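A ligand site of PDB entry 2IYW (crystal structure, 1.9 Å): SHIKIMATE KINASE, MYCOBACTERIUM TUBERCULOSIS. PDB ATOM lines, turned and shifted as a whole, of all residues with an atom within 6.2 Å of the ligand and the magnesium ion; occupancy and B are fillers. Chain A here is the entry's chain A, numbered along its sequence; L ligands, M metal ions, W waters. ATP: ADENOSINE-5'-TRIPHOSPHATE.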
ATOM      1  N   GLY A   9     -19.989   4.564   1.353  1.00  0.00           N
ATOM      2  CA  GLY A   9     -20.212   5.316   0.123  1.00  0.00           C
ATOM      3  C   GLY A   9     -21.259   6.393   0.272  1.00  0.00           C
ATOM      4  O   GLY A   9     -21.976   6.431   1.268  1.00  0.00           O
ATOM      5  N   LEU A  10     -21.367   7.245  -0.731  1.00  0.00           N
ATOM      6  CA  LEU A  10     -22.369   8.317  -0.723  1.00  0.00           C
ATOM      7  C   LEU A  10     -23.797   7.815  -0.888  1.00  0.00           C
ATOM      8  O   LEU A  10     -24.032   6.632  -1.190  1.00  0.00           O
ATOM      9  CB  LEU A  10     -22.068   9.276  -1.865  1.00  0.00           C
ATOM     10  CG  LEU A  10     -20.750  10.025  -1.765  1.00  0.00           C
ATOM     11  CD1 LEU A  10     -20.390  10.659  -3.129  1.00  0.00           C
ATOM     12  CD2 LEU A  10     -20.844  11.067  -0.684  1.00  0.00           C
ATOM     13  N   PRO A  11     -24.784   8.719  -0.719  1.00  0.00           N
ATOM     14  CA  PRO A  11     -26.164   8.317  -0.980  1.00  0.00           C
ATOM     15  C   PRO A  11     -26.322   7.892  -2.442  1.00  0.00           C
ATOM     16  O   PRO A  11     -25.798   8.529  -3.351  1.00  0.00           O
ATOM     17  CB  PRO A  11     -26.989   9.583  -0.660  1.00  0.00           C
ATOM     18  CG  PRO A  11     -26.078  10.432   0.185  1.00  0.00           C
ATOM     19  CD  PRO A  11     -24.697  10.129  -0.308  1.00  0.00           C
ATOM     20  N   GLY A  12     -26.993   6.768  -2.640  1.00  0.00           N
ATOM     21  CA  GLY A  12     -27.181   6.195  -3.962  1.00  0.00           C
ATOM     22  C   GLY A  12     -26.043   5.337  -4.474  1.00  0.00           C
ATOM     23  O   GLY A  12     -26.153   4.769  -5.554  1.00  0.00           O
ATOM     24  N   SER A  13     -24.948   5.224  -3.710  1.00  0.00           N
ATOM     25  CA  SER A  13     -23.816   4.426  -4.155  1.00  0.00           C
ATOM     26  C   SER A  13     -24.119   2.921  -4.205  1.00  0.00           C
ATOM     27  O   SER A  13     -23.438   2.166  -4.904  1.00  0.00           O
ATOM     28  CB  SER A  13     -22.579   4.674  -3.278  1.00  0.00           C
ATOM     29  OG  SER A  13     -22.795   4.376  -1.921  1.00  0.00           O
ATOM     30  N   GLY A  14     -25.120   2.482  -3.455  1.00  0.00           N
ATOM     31  CA  GLY A  14     -25.543   1.086  -3.468  1.00  0.00           C
ATOM     32  C   GLY A  14     -25.386   0.327  -2.161  1.00  0.00           C
ATOM     33  O   GLY A  14     -25.428  -0.898  -2.145  1.00  0.00           O
ATOM     34  N   LYS A  15     -25.229   1.045  -1.058  1.00  0.00           N
ATOM     35  CA  LYS A  15     -25.026   0.367   0.249  1.00  0.00           C
ATOM     36  C   LYS A  15     -26.154  -0.647   0.560  1.00  0.00           C
ATOM     37  O   LYS A  15     -25.894  -1.762   1.004  1.00  0.00           O
ATOM     38  CB  LYS A  15     -24.883   1.389   1.370  1.00  0.00           C
ATOM     39  CG  LYS A  15     -23.613   2.223   1.270  1.00  0.00           C
ATOM     40  CD  LYS A  15     -23.497   3.222   2.426  1.00  0.00           C
ATOM     41  CE  LYS A  15     -24.613   4.252   2.485  1.00  0.00           C
ATOM     42  NZ  LYS A  15     -24.842   5.007   1.191  1.00  0.00           N
ATOM     43  N   SER A  16     -27.401  -0.275   0.265  1.00  0.00           N
ATOM     44  CA  SER A  16     -28.530  -1.181   0.513  1.00  0.00           C
ATOM     45  C   SER A  16     -28.604  -2.301  -0.522  1.00  0.00           C
ATOM     46  O   SER A  16     -28.626  -3.486  -0.176  1.00  0.00           O
ATOM     47  CB  SER A  16     -29.829  -0.376   0.507  1.00  0.00           C
ATOM     48  OG  SER A  16     -29.822   0.541   1.576  1.00  0.00           O
ATOM     49  N   THR A  17     -28.633  -1.908  -1.788  1.00  0.00           N
ATOM     50  CA  THR A  17     -28.686  -2.856  -2.918  1.00  0.00           C
ATOM     51  C   THR A  17     -27.545  -3.864  -2.933  1.00  0.00           C
ATOM     52  O   THR A  17     -27.766  -5.074  -3.037  1.00  0.00           O
ATOM     53  CB  THR A  17     -28.658  -2.073  -4.241  1.00  0.00           C
ATOM     54  OG1 THR A  17     -29.709  -1.096  -4.225  1.00  0.00           O
ATOM     55  CG2 THR A  17     -28.830  -2.998  -5.419  1.00  0.00           C
ATOM     56  N   ILE A  18     -26.326  -3.352  -2.844  1.00  0.00           N
ATOM     57  CA  ILE A  18     -25.143  -4.211  -2.813  1.00  0.00           C
ATOM     58  C   ILE A  18     -25.048  -5.004  -1.494  1.00  0.00           C
ATOM     59  O   ILE A  18     -24.638  -6.162  -1.501  1.00  0.00           O
ATOM     60  CB  ILE A  18     -23.857  -3.391  -3.047  1.00  0.00           C
ATOM     61  CG1 ILE A  18     -23.959  -2.612  -4.368  1.00  0.00           C
ATOM     62  CG2 ILE A  18     -22.616  -4.290  -3.018  1.00  0.00           C
ATOM     63  CD1 ILE A  18     -24.192  -3.460  -5.632  1.00  0.00           C
ATOM     64  N   ARG A  20     -27.584  -6.153   0.314  1.00  0.00           N
ATOM     65  CA  ARG A  20     -28.476  -7.307   0.199  1.00  0.00           C
ATOM     66  C   ARG A  20     -27.917  -8.360  -0.746  1.00  0.00           C
ATOM     67  O   ARG A  20     -27.854  -9.534  -0.395  1.00  0.00           O
ATOM     68  CB  ARG A  20     -29.849  -6.892  -0.326  1.00  0.00           C
ATOM     69  CG  ARG A  20     -30.658  -6.057   0.649  1.00  0.00           C
ATOM     70  CD  ARG A  20     -32.073  -5.828   0.111  1.00  0.00           C
ATOM     71  NE  ARG A  20     -32.140  -4.679  -0.796  1.00  0.00           N
ATOM     72  CZ  ARG A  20     -32.474  -3.440  -0.442  1.00  0.00           C
ATOM     73  NH1 ARG A  20     -32.790  -3.136   0.819  1.00  0.00           N
ATOM     74  NH2 ARG A  20     -32.492  -2.479  -1.353  1.00  0.00           N
ATOM     75  N   ASP A  32     -27.229  -2.938   8.914  1.00  0.00           N
ATOM     76  CA  ASP A  32     -27.055  -1.546   8.526  1.00  0.00           C
ATOM     77  C   ASP A  32     -27.015  -0.689   9.775  1.00  0.00           C
ATOM     78  O   ASP A  32     -27.931  -0.762  10.594  1.00  0.00           O
ATOM     79  CB  ASP A  32     -28.169  -1.073   7.623  1.00  0.00           C
ATOM     80  CG  ASP A  32     -27.991   0.353   7.211  1.00  0.00           C
ATOM     81  OD1 ASP A  32     -27.117   0.630   6.364  1.00  0.00           O
ATOM     82  OD2 ASP A  32     -28.697   1.212   7.787  1.00  0.00           O
ATOM     83  N   GLY A  80     -23.862   7.153   6.142  1.00  0.00           N
ATOM     84  CA  GLY A  80     -22.979   8.003   5.330  1.00  0.00           C
ATOM     85  C   GLY A  80     -21.955   8.844   6.084  1.00  0.00           C
ATOM     86  O   GLY A  80     -20.839   9.063   5.598  1.00  0.00           O
ATOM     87  N   LEU A 100     -17.884   1.898  -2.247  1.00  0.00           N
ATOM     88  CA  LEU A 100     -18.695   1.954  -3.470  1.00  0.00           C
ATOM     89  C   LEU A 100     -18.640   3.377  -4.028  1.00  0.00           C
ATOM     90  O   LEU A 100     -19.244   4.304  -3.467  1.00  0.00           O
ATOM     91  CB  LEU A 100     -20.147   1.559  -3.154  1.00  0.00           C
ATOM     92  CG  LEU A 100     -20.401   0.224  -2.459  1.00  0.00           C
ATOM     93  CD1 LEU A 100     -21.880   0.048  -2.092  1.00  0.00           C
ATOM     94  CD2 LEU A 100     -19.933  -0.936  -3.317  1.00  0.00           C
ATOM     95  N   ARG A 109     -28.960  11.221  -9.748  1.00  0.00           N
ATOM     96  CA  ARG A 109     -29.916  10.407 -10.496  1.00  0.00           C
ATOM     97  C   ARG A 109     -30.472   9.264  -9.658  1.00  0.00           C
ATOM     98  O   ARG A 109     -31.679   9.034  -9.612  1.00  0.00           O
ATOM     99  CB  ARG A 109     -29.276   9.814 -11.740  1.00  0.00           C
ATOM    100  CG  ARG A 109     -30.262   9.102 -12.634  1.00  0.00           C
ATOM    101  CD  ARG A 109     -29.570   8.446 -13.807  1.00  0.00           C
ATOM    102  NE  ARG A 109     -28.742   7.286 -13.444  1.00  0.00           N
ATOM    103  CZ  ARG A 109     -29.202   6.083 -13.076  1.00  0.00           C
ATOM    104  NH1 ARG A 109     -30.486   5.851 -12.945  1.00  0.00           N
ATOM    105  NH2 ARG A 109     -28.344   5.112 -12.839  1.00  0.00           N
ATOM    106  N   ARG A 110     -29.563   8.552  -8.983  1.00  0.00           N
ATOM    107  CA  ARG A 110     -29.916   7.376  -8.175  1.00  0.00           C
ATOM    108  C   ARG A 110     -30.551   7.684  -6.817  1.00  0.00           C
ATOM    109  O   ARG A 110     -30.923   6.771  -6.080  1.00  0.00           O
ATOM    110  CB  ARG A 110     -28.688   6.448  -8.062  1.00  0.00           C
ATOM    111  CG  ARG A 110     -28.495   5.623  -9.342  1.00  0.00           C
ATOM    112  CD  ARG A 110     -27.083   5.205  -9.706  1.00  0.00           C
ATOM    113  NE  ARG A 110     -26.395   4.485  -8.639  1.00  0.00           N
ATOM    114  CZ  ARG A 110     -25.282   3.770  -8.801  1.00  0.00           C
ATOM    115  NH1 ARG A 110     -24.707   3.641  -9.988  1.00  0.00           N
ATOM    116  NH2 ARG A 110     -24.719   3.192  -7.751  1.00  0.00           N
ATOM    117  N   THR A 111     -30.688   8.967  -6.488  1.00  0.00           N
ATOM    118  CA  THR A 111     -31.396   9.367  -5.284  1.00  0.00           C
ATOM    119  C   THR A 111     -32.607  10.272  -5.590  1.00  0.00           C
ATOM    120  O   THR A 111     -32.955  11.135  -4.799  1.00  0.00           O
ATOM    121  CB  THR A 111     -30.454  10.021  -4.259  1.00  0.00           C
ATOM    122  OG1 THR A 111     -29.763  11.145  -4.841  1.00  0.00           O
ATOM    123  CG2 THR A 111     -29.435   9.016  -3.770  1.00  0.00           C
ATOM    124  N   THR A 150     -18.960   2.119  -9.248  1.00  0.00           N
ATOM    125  CA  THR A 150     -20.327   1.658  -9.545  1.00  0.00           C
ATOM    126  C   THR A 150     -20.986   2.474 -10.658  1.00  0.00           C
ATOM    127  O   THR A 150     -22.142   2.220 -10.986  1.00  0.00           O
ATOM    128  CB  THR A 150     -21.233   1.701  -8.321  1.00  0.00           C
ATOM    129  OG1 THR A 150     -21.602   3.049  -8.029  1.00  0.00           O
ATOM    130  CG2 THR A 150     -20.543   1.048  -7.097  1.00  0.00           C
ATOM    131  N   ASN A 151     -20.288   3.453 -11.213  1.00  0.00           N
ATOM    132  CA  ASN A 151     -20.900   4.327 -12.223  1.00  0.00           C
ATOM    133  C   ASN A 151     -21.335   3.553 -13.476  1.00  0.00           C
ATOM    134  O   ASN A 151     -22.383   3.840 -14.042  1.00  0.00           O
ATOM    135  CB  ASN A 151     -19.973   5.468 -12.618  1.00  0.00           C
ATOM    136  CG  ASN A 151     -19.825   6.485 -11.534  1.00  0.00           C
ATOM    137  OD1 ASN A 151     -20.827   7.066 -11.077  1.00  0.00           O
ATOM    138  ND2 ASN A 151     -18.589   6.714 -11.099  1.00  0.00           N
ATOM    139  N   ARG A 153     -21.076  -0.117 -13.684  1.00  0.00           N
ATOM    140  CA  ARG A 153     -21.333  -1.517 -13.380  1.00  0.00           C
ATOM    141  C   ARG A 153     -22.703  -1.593 -12.762  1.00  0.00           C
ATOM    142  O   ARG A 153     -23.016  -0.831 -11.850  1.00  0.00           O
ATOM    143  CB  ARG A 153     -20.320  -2.058 -12.361  1.00  0.00           C
ATOM    144  CG  ARG A 153     -18.932  -2.243 -12.862  1.00  0.00           C
ATOM    145  CD  ARG A 153     -18.136  -3.078 -11.851  1.00  0.00           C
ATOM    146  NE  ARG A 153     -16.743  -3.246 -12.258  1.00  0.00           N
ATOM    147  CZ  ARG A 153     -15.734  -2.447 -11.903  1.00  0.00           C
ATOM    148  NH1 ARG A 153     -15.936  -1.402 -11.128  1.00  0.00           N
ATOM    149  NH2 ARG A 153     -14.510  -2.713 -12.348  1.00  0.00           N
ATOM    150  N   ASN A 154     -23.521  -2.535 -13.235  1.00  0.00           N
ATOM    151  CA  ASN A 154     -24.811  -2.810 -12.603  1.00  0.00           C
ATOM    152  C   ASN A 154     -24.569  -3.583 -11.287  1.00  0.00           C
ATOM    153  O   ASN A 154     -23.440  -4.024 -11.038  1.00  0.00           O
ATOM    154  CB  ASN A 154     -25.757  -3.559 -13.568  1.00  0.00           C
ATOM    155  CG  ASN A 154     -25.187  -4.885 -14.038  1.00  0.00           C
ATOM    156  OD1 ASN A 154     -24.802  -5.735 -13.249  1.00  0.00           O
ATOM    157  ND2 ASN A 154     -25.140  -5.067 -15.360  1.00  0.00           N
ATOM    158  N   PRO A 155     -25.601  -3.729 -10.427  1.00  0.00           N
ATOM    159  CA  PRO A 155     -25.354  -4.376  -9.114  1.00  0.00           C
ATOM    160  C   PRO A 155     -24.768  -5.793  -9.163  1.00  0.00           C
ATOM    161  O   PRO A 155     -23.897  -6.123  -8.356  1.00  0.00           O
ATOM    162  CB  PRO A 155     -26.746  -4.378  -8.474  1.00  0.00           C
ATOM    163  CG  PRO A 155     -27.418  -3.236  -9.080  1.00  0.00           C
ATOM    164  CD  PRO A 155     -26.990  -3.259 -10.523  1.00  0.00           C
ATOM    165  N   VAL A 158     -21.066  -5.406  -9.815  1.00  0.00           N
ATOM    166  CA  VAL A 158     -20.433  -4.913  -8.596  1.00  0.00           C
ATOM    167  C   VAL A 158     -20.235  -6.057  -7.590  1.00  0.00           C
ATOM    168  O   VAL A 158     -19.150  -6.203  -7.014  1.00  0.00           O
ATOM    169  CB  VAL A 158     -21.272  -3.756  -7.960  1.00  0.00           C
ATOM    170  CG1 VAL A 158     -20.711  -3.332  -6.603  1.00  0.00           C
ATOM    171  CG2 VAL A 158     -21.319  -2.558  -8.891  1.00  0.00           C
HETATM  172  PG  ATP L   1     -28.731   5.678   0.838  1.00  0.00           P
HETATM  173  O1G ATP L   1     -29.294   4.608   1.760  1.00  0.00           O
HETATM  174  O2G ATP L   1     -27.412   6.236   1.320  1.00  0.00           O
HETATM  175  O3G ATP L   1     -29.708   6.764   0.472  1.00  0.00           O
HETATM  176  PB  ATP L   1     -27.722   3.558  -0.803  1.00  0.00           P
HETATM  177  O1B ATP L   1     -28.347   2.536   0.124  1.00  0.00           O
HETATM  178  O2B ATP L   1     -26.207   3.701  -0.893  1.00  0.00           O
HETATM  179  O3B ATP L   1     -28.409   4.997  -0.587  1.00  0.00           O
HETATM  180  PA  ATP L   1     -29.361   2.248  -2.797  1.00  0.00           P
HETATM  181  O1A ATP L   1     -28.894   0.822  -2.670  1.00  0.00           O
HETATM  182  O2A ATP L   1     -30.608   2.678  -2.099  1.00  0.00           O
HETATM  183  O3A ATP L   1     -28.213   3.272  -2.329  1.00  0.00           O
HETATM  184  O5' ATP L   1     -29.464   2.547  -4.382  1.00  0.00           O
HETATM  185  C5' ATP L   1     -30.063   3.732  -4.888  1.00  0.00           C
HETATM  186  C4' ATP L   1     -30.642   3.477  -6.281  1.00  0.00           C
HETATM  187  O4' ATP L   1     -29.600   3.199  -7.222  1.00  0.00           O
HETATM  188  C3' ATP L   1     -31.599   2.300  -6.335  1.00  0.00           C
HETATM  189  O3' ATP L   1     -32.650   2.629  -7.254  1.00  0.00           O
HETATM  190  C2' ATP L   1     -30.749   1.173  -6.876  1.00  0.00           C
HETATM  191  O2' ATP L   1     -31.487   0.206  -7.601  1.00  0.00           O
HETATM  192  C1' ATP L   1     -29.791   1.908  -7.789  1.00  0.00           C
HETATM  193  N9  ATP L   1     -28.466   1.281  -7.889  1.00  0.00           N
HETATM  194  C8  ATP L   1     -27.726   0.830  -6.862  1.00  0.00           C
HETATM  195  N7  ATP L   1     -26.567   0.325  -7.318  1.00  0.00           N
HETATM  196  C5  ATP L   1     -26.547   0.484  -8.660  1.00  0.00           C
HETATM  197  C6  ATP L   1     -25.607   0.152  -9.748  1.00  0.00           C
HETATM  198  N6  ATP L   1     -24.420  -0.433  -9.492  1.00  0.00           N
HETATM  199  N1  ATP L   1     -25.977   0.469 -11.004  1.00  0.00           N
HETATM  200  C2  ATP L   1     -27.149   1.064 -11.273  1.00  0.00           C
HETATM  201  N3  ATP L   1     -28.051   1.378 -10.328  1.00  0.00           N
HETATM  202  C4  ATP L   1     -27.809   1.110  -9.031  1.00  0.00           C
HETATM  203 MG    MG M   1     -29.508   2.569   1.776  1.00  0.00          MG
HETATM  204  O   HOH W   1     -35.817   2.007  -8.034  1.00  0.00           O
HETATM  205  O   HOH W   2     -30.887   8.982  -0.387  1.00  0.00           O
HETATM  206  O   HOH W   3     -23.840  -0.132  -6.618  1.00  0.00           O
HETATM  207  O   HOH W   4     -30.181   2.823 -11.487  1.00  0.00           O
HETATM  208  O   HOH W   5     -28.034   2.263   3.162  1.00  0.00           O
HETATM  209  O   HOH W   6     -32.066   4.364  -9.671  1.00  0.00           O
HETATM  210  O   HOH W   7     -27.205   8.155   3.079  1.00  0.00           O
HETATM  211  O   HOH W   8     -30.208   5.701   4.663  1.00  0.00           O
HETATM  212  O   HOH W   9     -32.356  -1.542  -5.026  1.00  0.00           O
HETATM  213  O   HOH W  10     -32.566   5.659   1.339  1.00  0.00           O
HETATM  214  O   HOH W  11     -31.537   6.005  -1.892  1.00  0.00           O
HETATM  215  O   HOH W  12     -31.098   2.728   0.496  1.00  0.00           O
HETATM  216  O   HOH W  13     -30.867   2.782   3.304  1.00  0.00           O
HETATM  217  O   HOH W  14     -32.198   0.171  -2.065  1.00  0.00           O
HETATM  218  O   HOH W  15     -24.366   1.509 -13.041  1.00  0.00           O
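The backbone NH (N) of Ser 16 lies within hydrogen-bond range of an oxygen (O1A) of the ligand (3.5 Å). N of Thr 17 lies within hydrogen-bond range of O1A of the ligand, 2.9 Å away. O1A of the ligand lies within hydrogen-bond range of OG1 of Thr 17. The backbone carbonyl oxygen (O) of Arg 153 sits at hydrogen-bond distance from a nitrogen (N6) of the ligand (2.8 Å). N of Lys 15 lies within hydrogen-bond range of O2B of the ligand, 2.8 Å away. The side-chain amino group (NZ) of Lys 15 lies within salt-bridge range of an oxygen (O2B) of the ligand, at 2.8 Å. The backbone NH (N) of Gly 14 sits at hydrogen-bond distance from an oxygen (O2B) of the ligand, at 3.0 Å. N of Gly 12 sits at hydrogen-bond distance from O3B of the ligand (3.1 Å). The guanidinium group (NH2) of Arg 110 sits close to a nitrogen (N7) of the ligand. An oxygen (O2B) of the ligand sits at hydrogen-bond distance from the backbone NH of Ser 13 (3.4 Å).
The side-chain amino group (NZ) of Lys 15 is in hydrogen-bond range of the backbone carbonyl oxygen (O) of Leu 10, 3.0 Å away. The side-chain amino group (NZ) of Lys 15 lies within hydrogen-bond range of the backbone carbonyl oxygen (O) of Gly 9. The backbone carbonyl oxygen (O) of Gly 12 is in hydrogen-bond range of the guanidinium group (NH2) of Arg 110. The backbone carbonyl oxygen of Ser 13 lies within hydrogen-bond range of the guanidinium group of Arg 110 (3.3 Å). The guanidinium group (NH1) of Arg 110 sits at hydrogen-bond distance from the backbone carbonyl oxygen (O) of Thr 150, at 3.1 Å. The side-chain hydroxyl (OG) of Ser 13 sits at hydrogen-bond distance from the backbone carbonyl oxygen (O) of Leu 10 (2.7 Å).
Residues that only touch the ligand: Leu 10, Pro 11, Thr 150, Asn 154, Pro 155 and Val 158. Hydrophobic or aromatic side chains within 4 Å of the ligand: Pro 11, Pro 155 and Val 158.
Of the 23 residues printed, 1 comes within 4 Å of the magnesium ion. The nearest printed residue that does not touch the magnesium ion is Lys 15 (4.8 Å).
The magnesium ion is bound by an oxygen (O1B) of the ligand (2.0 Å), water W5 (2.0 Å), water W12 (2.0 Å), an oxygen (O1G) of the ligand (2.1 Å), water W13 (2.1 Å) and the side-chain hydroxyl (OG) of Ser 16 (2.1 Å). The magnesium ion has six donor atoms within binding distance.
Water W4 bridges a nitrogen (N3) of the ligand (2.8 Å) and the guanidinium group (NH2) of Arg 109 (3.2 Å). Water W3 bridges N7 of the ligand (2.9 Å) and O of Ser 13 (2.9 Å). Water W14 lies within hydrogen-bond range of NH2 of Arg 20 (2.8 Å) and O2A of the ligand (3.0 Å). Water W9 bridges the side-chain hydroxyl (OG1) of Thr 17 (2.8 Å) and an oxygen (O2') of the ligand (3.2 Å).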
